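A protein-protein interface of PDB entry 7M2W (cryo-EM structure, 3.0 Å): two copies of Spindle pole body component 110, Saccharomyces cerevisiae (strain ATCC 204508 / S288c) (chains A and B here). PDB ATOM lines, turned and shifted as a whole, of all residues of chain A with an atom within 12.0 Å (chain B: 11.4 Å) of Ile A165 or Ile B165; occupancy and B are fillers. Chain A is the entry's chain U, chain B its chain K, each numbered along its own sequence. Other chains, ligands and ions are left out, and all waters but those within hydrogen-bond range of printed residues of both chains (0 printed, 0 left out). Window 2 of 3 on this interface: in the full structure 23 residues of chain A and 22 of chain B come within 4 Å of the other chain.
Ile A165 touches just these residues of chain B: Ile B165 (3.5 Å) and Leu B168 (3.98 Å).
Of the printed residues of chain A, Ile B165 touches Ile A165 (3.5 Å).
No residue of chain B comes within 4 Å of Glu A164.
Lys A169 touches just one residue of chain B: Leu B168 (3.9 Å).
No residue of chain A comes within 4 Å of Asn B163.
No residue of chain A comes within 4 Å of Glu B164.
No residue of chain A comes within 4 Å of Lys B166.
No residue of chain A comes within 4 Å of Ser B167.
Leu B168 touches three residues of chain A.
Of the printed residues of chain A, Glu B171 touches Ile A172 (3.6 Å) and Arg A176 (2.7 Å).
Of the printed residues of chain B, Arg A176 touches Glu B171 (2.7 Å).
Of the printed residues of chain A, Ile B172 touches Leu A168, Glu A171, Ile A172 and Leu A175.
Of the printed residues of chain B, Leu A175 touches Ile B172.
Of the printed residues of chain B, Glu A171 touches Ile B172 (3.8 Å).
The nearest residue of chain B that does not touch Ile A165 is Lys B166 (4.4 Å).
The nearest residue of chain A that does not touch Ile B165 is Leu A168 (5.1 Å).
OE2 of Glu B171 lies within salt-bridge range of NH2 of Arg A176, at 2.7 Å.
Ile B165 touches its own counterpart, Ile A165.
Ile A165 touches Leu B168, but with the chains exchanged Leu A168 does not touch Ile B165 (5.1 Å).
Lys A169 touches Leu B168, but with the chains exchanged Leu A168 does not touch Lys B169 (4.4 Å).
Ile B172 touches its own counterpart, Ile A172.
Of the 10 pairs that touch across the chains among the printed residues, 6 have their exchanged pair printed and touching as well.
Hydrophobic or aromatic side chains of chain A that line the printed part of chain B: Ile A165, Leu A168, Ile A172 and Leu A175.
Of the 12 printed residues of chain B, 4 touch a printed residue of chain A.
Hydrophobic or aromatic side chains of chain B within 4 Å of the printed part of chain A: Leu B168 and Ile B172.
Among the printed residues, Asp or Glu carboxylates within 4 Å of a Lys or Arg side-chain nitrogen of the other chain: Arg A176 with Glu B171.
Among the printed residues, merely in contact across the chains: Ile A165 with Ile B165 (3.5 Å), Ile A165 with Leu B168 (3.98 Å), Leu A168 with Ile B172 (3.6 Å), Lys A169 with Leu B168 (3.9 Å), Glu A171 with Ile B172 (3.8 Å), Ile A172 with Leu B168 (3.9 Å), Ile A172 with Glu B171 (3.6 Å), Ile A172 with Ile B172 (3.4 Å) and Leu A175 with Ile B172 (3.9 Å).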
ATOM      1  N   GLU A 164      -1.312 -19.556  -7.118  1.00  0.00           N
ATOM      2  CA  GLU A 164      -2.497 -20.457  -7.064  1.00  0.00           C
ATOM      3  C   GLU A 164      -2.304 -21.787  -7.816  1.00  0.00           C
ATOM      4  O   GLU A 164      -2.343 -22.836  -7.182  1.00  0.00           O
ATOM      5  CB  GLU A 164      -3.827 -19.738  -7.391  1.00  0.00           C
ATOM      6  CG  GLU A 164      -4.234 -19.442  -8.850  1.00  0.00           C
ATOM      7  CD  GLU A 164      -3.235 -18.583  -9.635  1.00  0.00           C
ATOM      8  OE1 GLU A 164      -2.048 -18.968  -9.695  1.00  0.00           O
ATOM      9  OE2 GLU A 164      -3.630 -17.541 -10.186  1.00  0.00           O
ATOM     10  N   ILE A 165      -2.078 -21.805  -9.138  1.00  0.00           N
ATOM     11  CA  ILE A 165      -2.132 -23.041  -9.956  1.00  0.00           C
ATOM     12  C   ILE A 165      -1.131 -24.124  -9.509  1.00  0.00           C
ATOM     13  O   ILE A 165      -1.486 -25.304  -9.510  1.00  0.00           O
ATOM     14  CB  ILE A 165      -1.977 -22.700 -11.463  1.00  0.00           C
ATOM     15  CG1 ILE A 165      -3.128 -21.824 -12.013  1.00  0.00           C
ATOM     16  CG2 ILE A 165      -1.835 -23.956 -12.340  1.00  0.00           C
ATOM     17  CD1 ILE A 165      -4.543 -22.406 -11.904  1.00  0.00           C
ATOM     18  N   LYS A 166       0.074 -23.757  -9.048  1.00  0.00           N
ATOM     19  CA  LYS A 166       1.082 -24.715  -8.615  1.00  0.00           C
ATOM     20  C   LYS A 166       0.585 -25.497  -7.408  1.00  0.00           C
ATOM     21  O   LYS A 166       0.829 -26.705  -7.293  1.00  0.00           O
ATOM     22  CB  LYS A 166       2.393 -24.007  -8.283  1.00  0.00           C
ATOM     23  CG  LYS A 166       3.126 -23.455  -9.496  1.00  0.00           C
ATOM     24  CD  LYS A 166       4.413 -22.741  -9.090  1.00  0.00           C
ATOM     25  CE  LYS A 166       5.150 -22.185 -10.305  1.00  0.00           C
ATOM     26  NZ  LYS A 166       6.388 -21.444  -9.918  1.00  0.00           N
ATOM     27  N   SER A 167      -0.134 -24.811  -6.518  1.00  0.00           N
ATOM     28  CA  SER A 167      -0.654 -25.441  -5.320  1.00  0.00           C
ATOM     29  C   SER A 167      -1.717 -26.459  -5.693  1.00  0.00           C
ATOM     30  O   SER A 167      -1.755 -27.559  -5.127  1.00  0.00           O
ATOM     31  CB  SER A 167      -1.256 -24.399  -4.392  1.00  0.00           C
ATOM     32  OG  SER A 167      -0.278 -23.517  -3.908  1.00  0.00           O
ATOM     33  N   LEU A 168      -2.595 -26.118  -6.645  1.00  0.00           N
ATOM     34  CA  LEU A 168      -3.655 -27.014  -7.107  1.00  0.00           C
ATOM     35  C   LEU A 168      -3.063 -28.271  -7.756  1.00  0.00           C
ATOM     36  O   LEU A 168      -3.455 -29.385  -7.422  1.00  0.00           O
ATOM     37  CB  LEU A 168      -4.597 -26.268  -8.072  1.00  0.00           C
ATOM     38  CG  LEU A 168      -5.252 -24.996  -7.501  1.00  0.00           C
ATOM     39  CD1 LEU A 168      -6.242 -24.428  -8.509  1.00  0.00           C
ATOM     40  CD2 LEU A 168      -6.002 -25.226  -6.195  1.00  0.00           C
ATOM     41  N   LYS A 169      -2.048 -28.111  -8.614  1.00  0.00           N
ATOM     42  CA  LYS A 169      -1.311 -29.240  -9.201  1.00  0.00           C
ATOM     43  C   LYS A 169      -0.654 -30.125  -8.134  1.00  0.00           C
ATOM     44  O   LYS A 169      -0.700 -31.345  -8.265  1.00  0.00           O
ATOM     45  CB  LYS A 169      -0.284 -28.729 -10.224  1.00  0.00           C
ATOM     46  CG  LYS A 169      -0.966 -28.191 -11.492  1.00  0.00           C
ATOM     47  CD  LYS A 169       0.066 -27.753 -12.537  1.00  0.00           C
ATOM     48  CE  LYS A 169      -0.632 -27.307 -13.825  1.00  0.00           C
ATOM     49  NZ  LYS A 169       0.344 -26.945 -14.879  1.00  0.00           N
ATOM     50  N   HIS A 170      -0.114 -29.556  -7.051  1.00  0.00           N
ATOM     51  CA  HIS A 170       0.442 -30.341  -5.967  1.00  0.00           C
ATOM     52  C   HIS A 170      -0.637 -31.194  -5.313  1.00  0.00           C
ATOM     53  O   HIS A 170      -0.443 -32.399  -5.102  1.00  0.00           O
ATOM     54  CB  HIS A 170       1.061 -29.459  -4.886  1.00  0.00           C
ATOM     55  CG  HIS A 170       1.671 -30.274  -3.820  1.00  0.00           C
ATOM     56  ND1 HIS A 170       2.918 -30.849  -3.946  1.00  0.00           N
ATOM     57  CD2 HIS A 170       1.184 -30.683  -2.631  1.00  0.00           C
ATOM     58  CE1 HIS A 170       3.172 -31.567  -2.868  1.00  0.00           C
ATOM     59  NE2 HIS A 170       2.135 -31.487  -2.063  1.00  0.00           N
ATOM     60  N   GLU A 171      -1.785 -30.582  -4.991  1.00  0.00           N
ATOM     61  CA  GLU A 171      -2.836 -31.335  -4.319  1.00  0.00           C
ATOM     62  C   GLU A 171      -3.324 -32.471  -5.198  1.00  0.00           C
ATOM     63  O   GLU A 171      -3.603 -33.563  -4.698  1.00  0.00           O
ATOM     64  CB  GLU A 171      -4.020 -30.448  -3.952  1.00  0.00           C
ATOM     65  CG  GLU A 171      -3.739 -29.427  -2.859  1.00  0.00           C
ATOM     66  CD  GLU A 171      -4.965 -28.627  -2.467  1.00  0.00           C
ATOM     67  OE1 GLU A 171      -6.061 -29.088  -2.720  1.00  0.00           O
ATOM     68  OE2 GLU A 171      -4.807 -27.565  -1.920  1.00  0.00           O
ATOM     69  N   ILE A 172      -3.462 -32.231  -6.509  1.00  0.00           N
ATOM     70  CA  ILE A 172      -3.853 -33.260  -7.476  1.00  0.00           C
ATOM     71  C   ILE A 172      -2.864 -34.422  -7.414  1.00  0.00           C
ATOM     72  O   ILE A 172      -3.300 -35.572  -7.323  1.00  0.00           O
ATOM     73  CB  ILE A 172      -3.975 -32.665  -8.900  1.00  0.00           C
ATOM     74  CG1 ILE A 172      -5.253 -31.809  -8.971  1.00  0.00           C
ATOM     75  CG2 ILE A 172      -4.008 -33.755  -9.984  1.00  0.00           C
ATOM     76  CD1 ILE A 172      -5.414 -30.966 -10.235  1.00  0.00           C
ATOM     77  N   LYS A 173      -1.550 -34.155  -7.413  1.00  0.00           N
ATOM     78  CA  LYS A 173      -0.582 -35.233  -7.372  1.00  0.00           C
ATOM     79  C   LYS A 173      -0.689 -36.045  -6.083  1.00  0.00           C
ATOM     80  O   LYS A 173      -0.650 -37.284  -6.132  1.00  0.00           O
ATOM     81  CB  LYS A 173       0.831 -34.676  -7.510  1.00  0.00           C
ATOM     82  CG  LYS A 173       1.156 -34.143  -8.893  1.00  0.00           C
ATOM     83  CD  LYS A 173       2.567 -33.564  -8.959  1.00  0.00           C
ATOM     84  CE  LYS A 173       2.871 -33.006 -10.347  1.00  0.00           C
ATOM     85  NZ  LYS A 173       4.234 -32.401 -10.424  1.00  0.00           N
ATOM     86  N   GLU A 174      -0.877 -35.376  -4.935  1.00  0.00           N
ATOM     87  CA  GLU A 174      -0.993 -36.130  -3.692  1.00  0.00           C
ATOM     88  C   GLU A 174      -2.246 -36.986  -3.682  1.00  0.00           C
ATOM     89  O   GLU A 174      -2.202 -38.151  -3.269  1.00  0.00           O
ATOM     90  CB  GLU A 174      -1.029 -35.212  -2.460  1.00  0.00           C
ATOM     91  CG  GLU A 174       0.284 -34.520  -2.094  1.00  0.00           C
ATOM     92  CD  GLU A 174       0.138 -33.621  -0.863  1.00  0.00           C
ATOM     93  OE1 GLU A 174      -0.976 -33.324  -0.509  1.00  0.00           O
ATOM     94  OE2 GLU A 174       1.142 -33.260  -0.266  1.00  0.00           O
ATOM     95  N   LEU A 175      -3.383 -36.446  -4.132  1.00  0.00           N
ATOM     96  CA  LEU A 175      -4.655 -37.169  -4.149  1.00  0.00           C
ATOM     97  C   LEU A 175      -4.618 -38.359  -5.115  1.00  0.00           C
ATOM     98  O   LEU A 175      -5.078 -39.447  -4.771  1.00  0.00           O
ATOM     99  CB  LEU A 175      -5.787 -36.202  -4.528  1.00  0.00           C
ATOM    100  CG  LEU A 175      -6.113 -35.157  -3.448  1.00  0.00           C
ATOM    101  CD1 LEU A 175      -6.914 -34.013  -4.062  1.00  0.00           C
ATOM    102  CD2 LEU A 175      -6.940 -35.770  -2.320  1.00  0.00           C
ATOM    103  N   ARG A 176      -4.013 -38.194  -6.299  1.00  0.00           N
ATOM    104  CA  ARG A 176      -3.785 -39.299  -7.243  1.00  0.00           C
ATOM    105  C   ARG A 176      -2.954 -40.415  -6.616  1.00  0.00           C
ATOM    106  O   ARG A 176      -3.295 -41.585  -6.768  1.00  0.00           O
ATOM    107  CB  ARG A 176      -3.078 -38.791  -8.504  1.00  0.00           C
ATOM    108  CG  ARG A 176      -4.006 -38.008  -9.438  1.00  0.00           C
ATOM    109  CD  ARG A 176      -3.180 -37.513 -10.623  1.00  0.00           C
ATOM    110  NE  ARG A 176      -3.975 -36.694 -11.548  1.00  0.00           N
ATOM    111  CZ  ARG A 176      -3.756 -36.553 -12.837  1.00  0.00           C
ATOM    112  NH1 ARG A 176      -2.864 -37.228 -13.491  1.00  0.00           N
ATOM    113  NH2 ARG A 176      -4.448 -35.719 -13.533  1.00  0.00           N
ATOM    114  N   TYR B 161     -11.506 -19.372 -26.957  1.00  0.00           N
ATOM    115  CA  TYR B 161     -10.617 -18.503 -26.178  1.00  0.00           C
ATOM    116  C   TYR B 161     -10.388 -18.968 -24.728  1.00  0.00           C
ATOM    117  O   TYR B 161     -11.237 -19.637 -24.138  1.00  0.00           O
ATOM    118  CB  TYR B 161     -11.167 -17.072 -26.230  1.00  0.00           C
ATOM    119  CG  TYR B 161     -10.225 -16.013 -25.693  1.00  0.00           C
ATOM    120  CD1 TYR B 161      -9.041 -15.719 -26.386  1.00  0.00           C
ATOM    121  CD2 TYR B 161     -10.527 -15.322 -24.509  1.00  0.00           C
ATOM    122  CE1 TYR B 161      -8.156 -14.743 -25.895  1.00  0.00           C
ATOM    123  CE2 TYR B 161      -9.644 -14.343 -24.016  1.00  0.00           C
ATOM    124  CZ  TYR B 161      -8.451 -14.057 -24.706  1.00  0.00           C
ATOM    125  OH  TYR B 161      -7.598 -13.107 -24.246  1.00  0.00           O
ATOM    126  N   ILE B 162      -9.252 -18.575 -24.142  1.00  0.00           N
ATOM    127  CA  ILE B 162      -8.799 -18.967 -22.794  1.00  0.00           C
ATOM    128  C   ILE B 162      -8.196 -17.784 -22.014  1.00  0.00           C
ATOM    129  O   ILE B 162      -7.695 -16.827 -22.604  1.00  0.00           O
ATOM    130  CB  ILE B 162      -7.800 -20.148 -22.865  1.00  0.00           C
ATOM    131  CG1 ILE B 162      -6.493 -19.797 -23.603  1.00  0.00           C
ATOM    132  CG2 ILE B 162      -8.460 -21.391 -23.469  1.00  0.00           C
ATOM    133  CD1 ILE B 162      -5.416 -20.878 -23.514  1.00  0.00           C
ATOM    134  N   ASN B 163      -8.211 -17.869 -20.679  1.00  0.00           N
ATOM    135  CA  ASN B 163      -7.663 -16.846 -19.775  1.00  0.00           C
ATOM    136  C   ASN B 163      -6.978 -17.401 -18.503  1.00  0.00           C
ATOM    137  O   ASN B 163      -6.031 -16.793 -18.013  1.00  0.00           O
ATOM    138  CB  ASN B 163      -8.782 -15.852 -19.404  1.00  0.00           C
ATOM    139  CG  ASN B 163      -9.800 -16.419 -18.425  1.00  0.00           C
ATOM    140  OD1 ASN B 163     -10.377 -17.476 -18.631  1.00  0.00           O
ATOM    141  ND2 ASN B 163     -10.022 -15.761 -17.316  1.00  0.00           N
ATOM    142  N   GLU B 164      -7.436 -18.527 -17.950  1.00  0.00           N
ATOM    143  CA  GLU B 164      -6.935 -19.123 -16.698  1.00  0.00           C
ATOM    144  C   GLU B 164      -7.266 -20.629 -16.605  1.00  0.00           C
ATOM    145  O   GLU B 164      -8.146 -21.119 -17.311  1.00  0.00           O
ATOM    146  CB  GLU B 164      -7.516 -18.355 -15.493  1.00  0.00           C
ATOM    147  CG  GLU B 164      -9.013 -18.624 -15.269  1.00  0.00           C
ATOM    148  CD  GLU B 164      -9.726 -17.487 -14.525  1.00  0.00           C
ATOM    149  OE1 GLU B 164     -10.885 -17.184 -14.890  1.00  0.00           O
ATOM    150  OE2 GLU B 164      -9.155 -16.920 -13.571  1.00  0.00           O
ATOM    151  N   ILE B 165      -6.598 -21.363 -15.706  1.00  0.00           N
ATOM    152  CA  ILE B 165      -6.773 -22.817 -15.508  1.00  0.00           C
ATOM    153  C   ILE B 165      -7.528 -23.134 -14.197  1.00  0.00           C
ATOM    154  O   ILE B 165      -7.227 -24.090 -13.487  1.00  0.00           O
ATOM    155  CB  ILE B 165      -5.446 -23.607 -15.684  1.00  0.00           C
ATOM    156  CG1 ILE B 165      -4.495 -23.046 -16.769  1.00  0.00           C
ATOM    157  CG2 ILE B 165      -5.752 -25.062 -16.062  1.00  0.00           C
ATOM    158  CD1 ILE B 165      -3.463 -22.062 -16.220  1.00  0.00           C
ATOM    159  N   LYS B 166      -8.522 -22.313 -13.830  1.00  0.00           N
ATOM    160  CA  LYS B 166      -9.261 -22.439 -12.551  1.00  0.00           C
ATOM    161  C   LYS B 166     -10.027 -23.755 -12.375  1.00  0.00           C
ATOM    162  O   LYS B 166     -10.323 -24.150 -11.251  1.00  0.00           O
ATOM    163  CB  LYS B 166     -10.177 -21.223 -12.318  1.00  0.00           C
ATOM    164  CG  LYS B 166     -11.362 -21.094 -13.292  1.00  0.00           C
ATOM    165  CD  LYS B 166     -12.230 -19.889 -12.898  1.00  0.00           C
ATOM    166  CE  LYS B 166     -13.400 -19.614 -13.852  1.00  0.00           C
ATOM    167  NZ  LYS B 166     -12.965 -19.043 -15.151  1.00  0.00           N
ATOM    168  N   SER B 167     -10.303 -24.472 -13.464  1.00  0.00           N
ATOM    169  CA  SER B 167     -11.015 -25.759 -13.468  1.00  0.00           C
ATOM    170  C   SER B 167     -10.347 -26.854 -12.620  1.00  0.00           C
ATOM    171  O   SER B 167     -11.030 -27.787 -12.200  1.00  0.00           O
ATOM    172  CB  SER B 167     -11.174 -26.259 -14.910  1.00  0.00           C
ATOM    173  OG  SER B 167     -11.814 -25.286 -15.715  1.00  0.00           O
ATOM    174  N   LEU B 168      -9.051 -26.741 -12.294  1.00  0.00           N
ATOM    175  CA  LEU B 168      -8.329 -27.728 -11.473  1.00  0.00           C
ATOM    176  C   LEU B 168      -8.984 -27.985 -10.105  1.00  0.00           C
ATOM    177  O   LEU B 168      -8.923 -29.108  -9.612  1.00  0.00           O
ATOM    178  CB  LEU B 168      -6.867 -27.290 -11.268  1.00  0.00           C
ATOM    179  CG  LEU B 168      -5.986 -27.231 -12.527  1.00  0.00           C
ATOM    180  CD1 LEU B 168      -4.577 -26.827 -12.122  1.00  0.00           C
ATOM    181  CD2 LEU B 168      -5.898 -28.549 -13.275  1.00  0.00           C
ATOM    182  N   LYS B 169      -9.672 -27.000  -9.508  1.00  0.00           N
ATOM    183  CA  LYS B 169     -10.399 -27.199  -8.238  1.00  0.00           C
ATOM    184  C   LYS B 169     -11.513 -28.251  -8.332  1.00  0.00           C
ATOM    185  O   LYS B 169     -11.790 -28.945  -7.360  1.00  0.00           O
ATOM    186  CB  LYS B 169     -10.897 -25.854  -7.679  1.00  0.00           C
ATOM    187  CG  LYS B 169     -12.126 -25.273  -8.395  1.00  0.00           C
ATOM    188  CD  LYS B 169     -12.487 -23.899  -7.822  1.00  0.00           C
ATOM    189  CE  LYS B 169     -13.747 -23.357  -8.494  1.00  0.00           C
ATOM    190  NZ  LYS B 169     -14.142 -22.045  -7.930  1.00  0.00           N
ATOM    191  N   HIS B 170     -12.114 -28.431  -9.506  1.00  0.00           N
ATOM    192  CA  HIS B 170     -13.134 -29.458  -9.728  1.00  0.00           C
ATOM    193  C   HIS B 170     -12.514 -30.854  -9.881  1.00  0.00           C
ATOM    194  O   HIS B 170     -13.020 -31.801  -9.287  1.00  0.00           O
ATOM    195  CB  HIS B 170     -14.003 -29.059 -10.923  1.00  0.00           C
ATOM    196  CG  HIS B 170     -14.744 -27.771 -10.671  1.00  0.00           C
ATOM    197  ND1 HIS B 170     -15.920 -27.637  -9.975  1.00  0.00           N
ATOM    198  CD2 HIS B 170     -14.310 -26.508 -10.961  1.00  0.00           C
ATOM    199  CE1 HIS B 170     -16.208 -26.332  -9.874  1.00  0.00           C
ATOM    200  NE2 HIS B 170     -15.252 -25.600 -10.466  1.00  0.00           N
ATOM    201  N   GLU B 171     -11.371 -30.988 -10.564  1.00  0.00           N
ATOM    202  CA  GLU B 171     -10.597 -32.241 -10.551  1.00  0.00           C
ATOM    203  C   GLU B 171     -10.156 -32.609  -9.124  1.00  0.00           C
ATOM    204  O   GLU B 171     -10.282 -33.762  -8.721  1.00  0.00           O
ATOM    205  CB  GLU B 171      -9.401 -32.149 -11.516  1.00  0.00           C
ATOM    206  CG  GLU B 171      -8.516 -33.406 -11.460  1.00  0.00           C
ATOM    207  CD  GLU B 171      -7.446 -33.494 -12.563  1.00  0.00           C
ATOM    208  OE1 GLU B 171      -7.522 -32.755 -13.568  1.00  0.00           O
ATOM    209  OE2 GLU B 171      -6.531 -34.336 -12.434  1.00  0.00           O
ATOM    210  N   ILE B 172      -9.729 -31.627  -8.322  1.00  0.00           N
ATOM    211  CA  ILE B 172      -9.428 -31.824  -6.898  1.00  0.00           C
ATOM    212  C   ILE B 172     -10.653 -32.339  -6.141  1.00  0.00           C
ATOM    213  O   ILE B 172     -10.543 -33.335  -5.430  1.00  0.00           O
ATOM    214  CB  ILE B 172      -8.870 -30.526  -6.273  1.00  0.00           C
ATOM    215  CG1 ILE B 172      -7.446 -30.296  -6.804  1.00  0.00           C
ATOM    216  CG2 ILE B 172      -8.862 -30.568  -4.736  1.00  0.00           C
ATOM    217  CD1 ILE B 172      -6.914 -28.881  -6.586  1.00  0.00           C
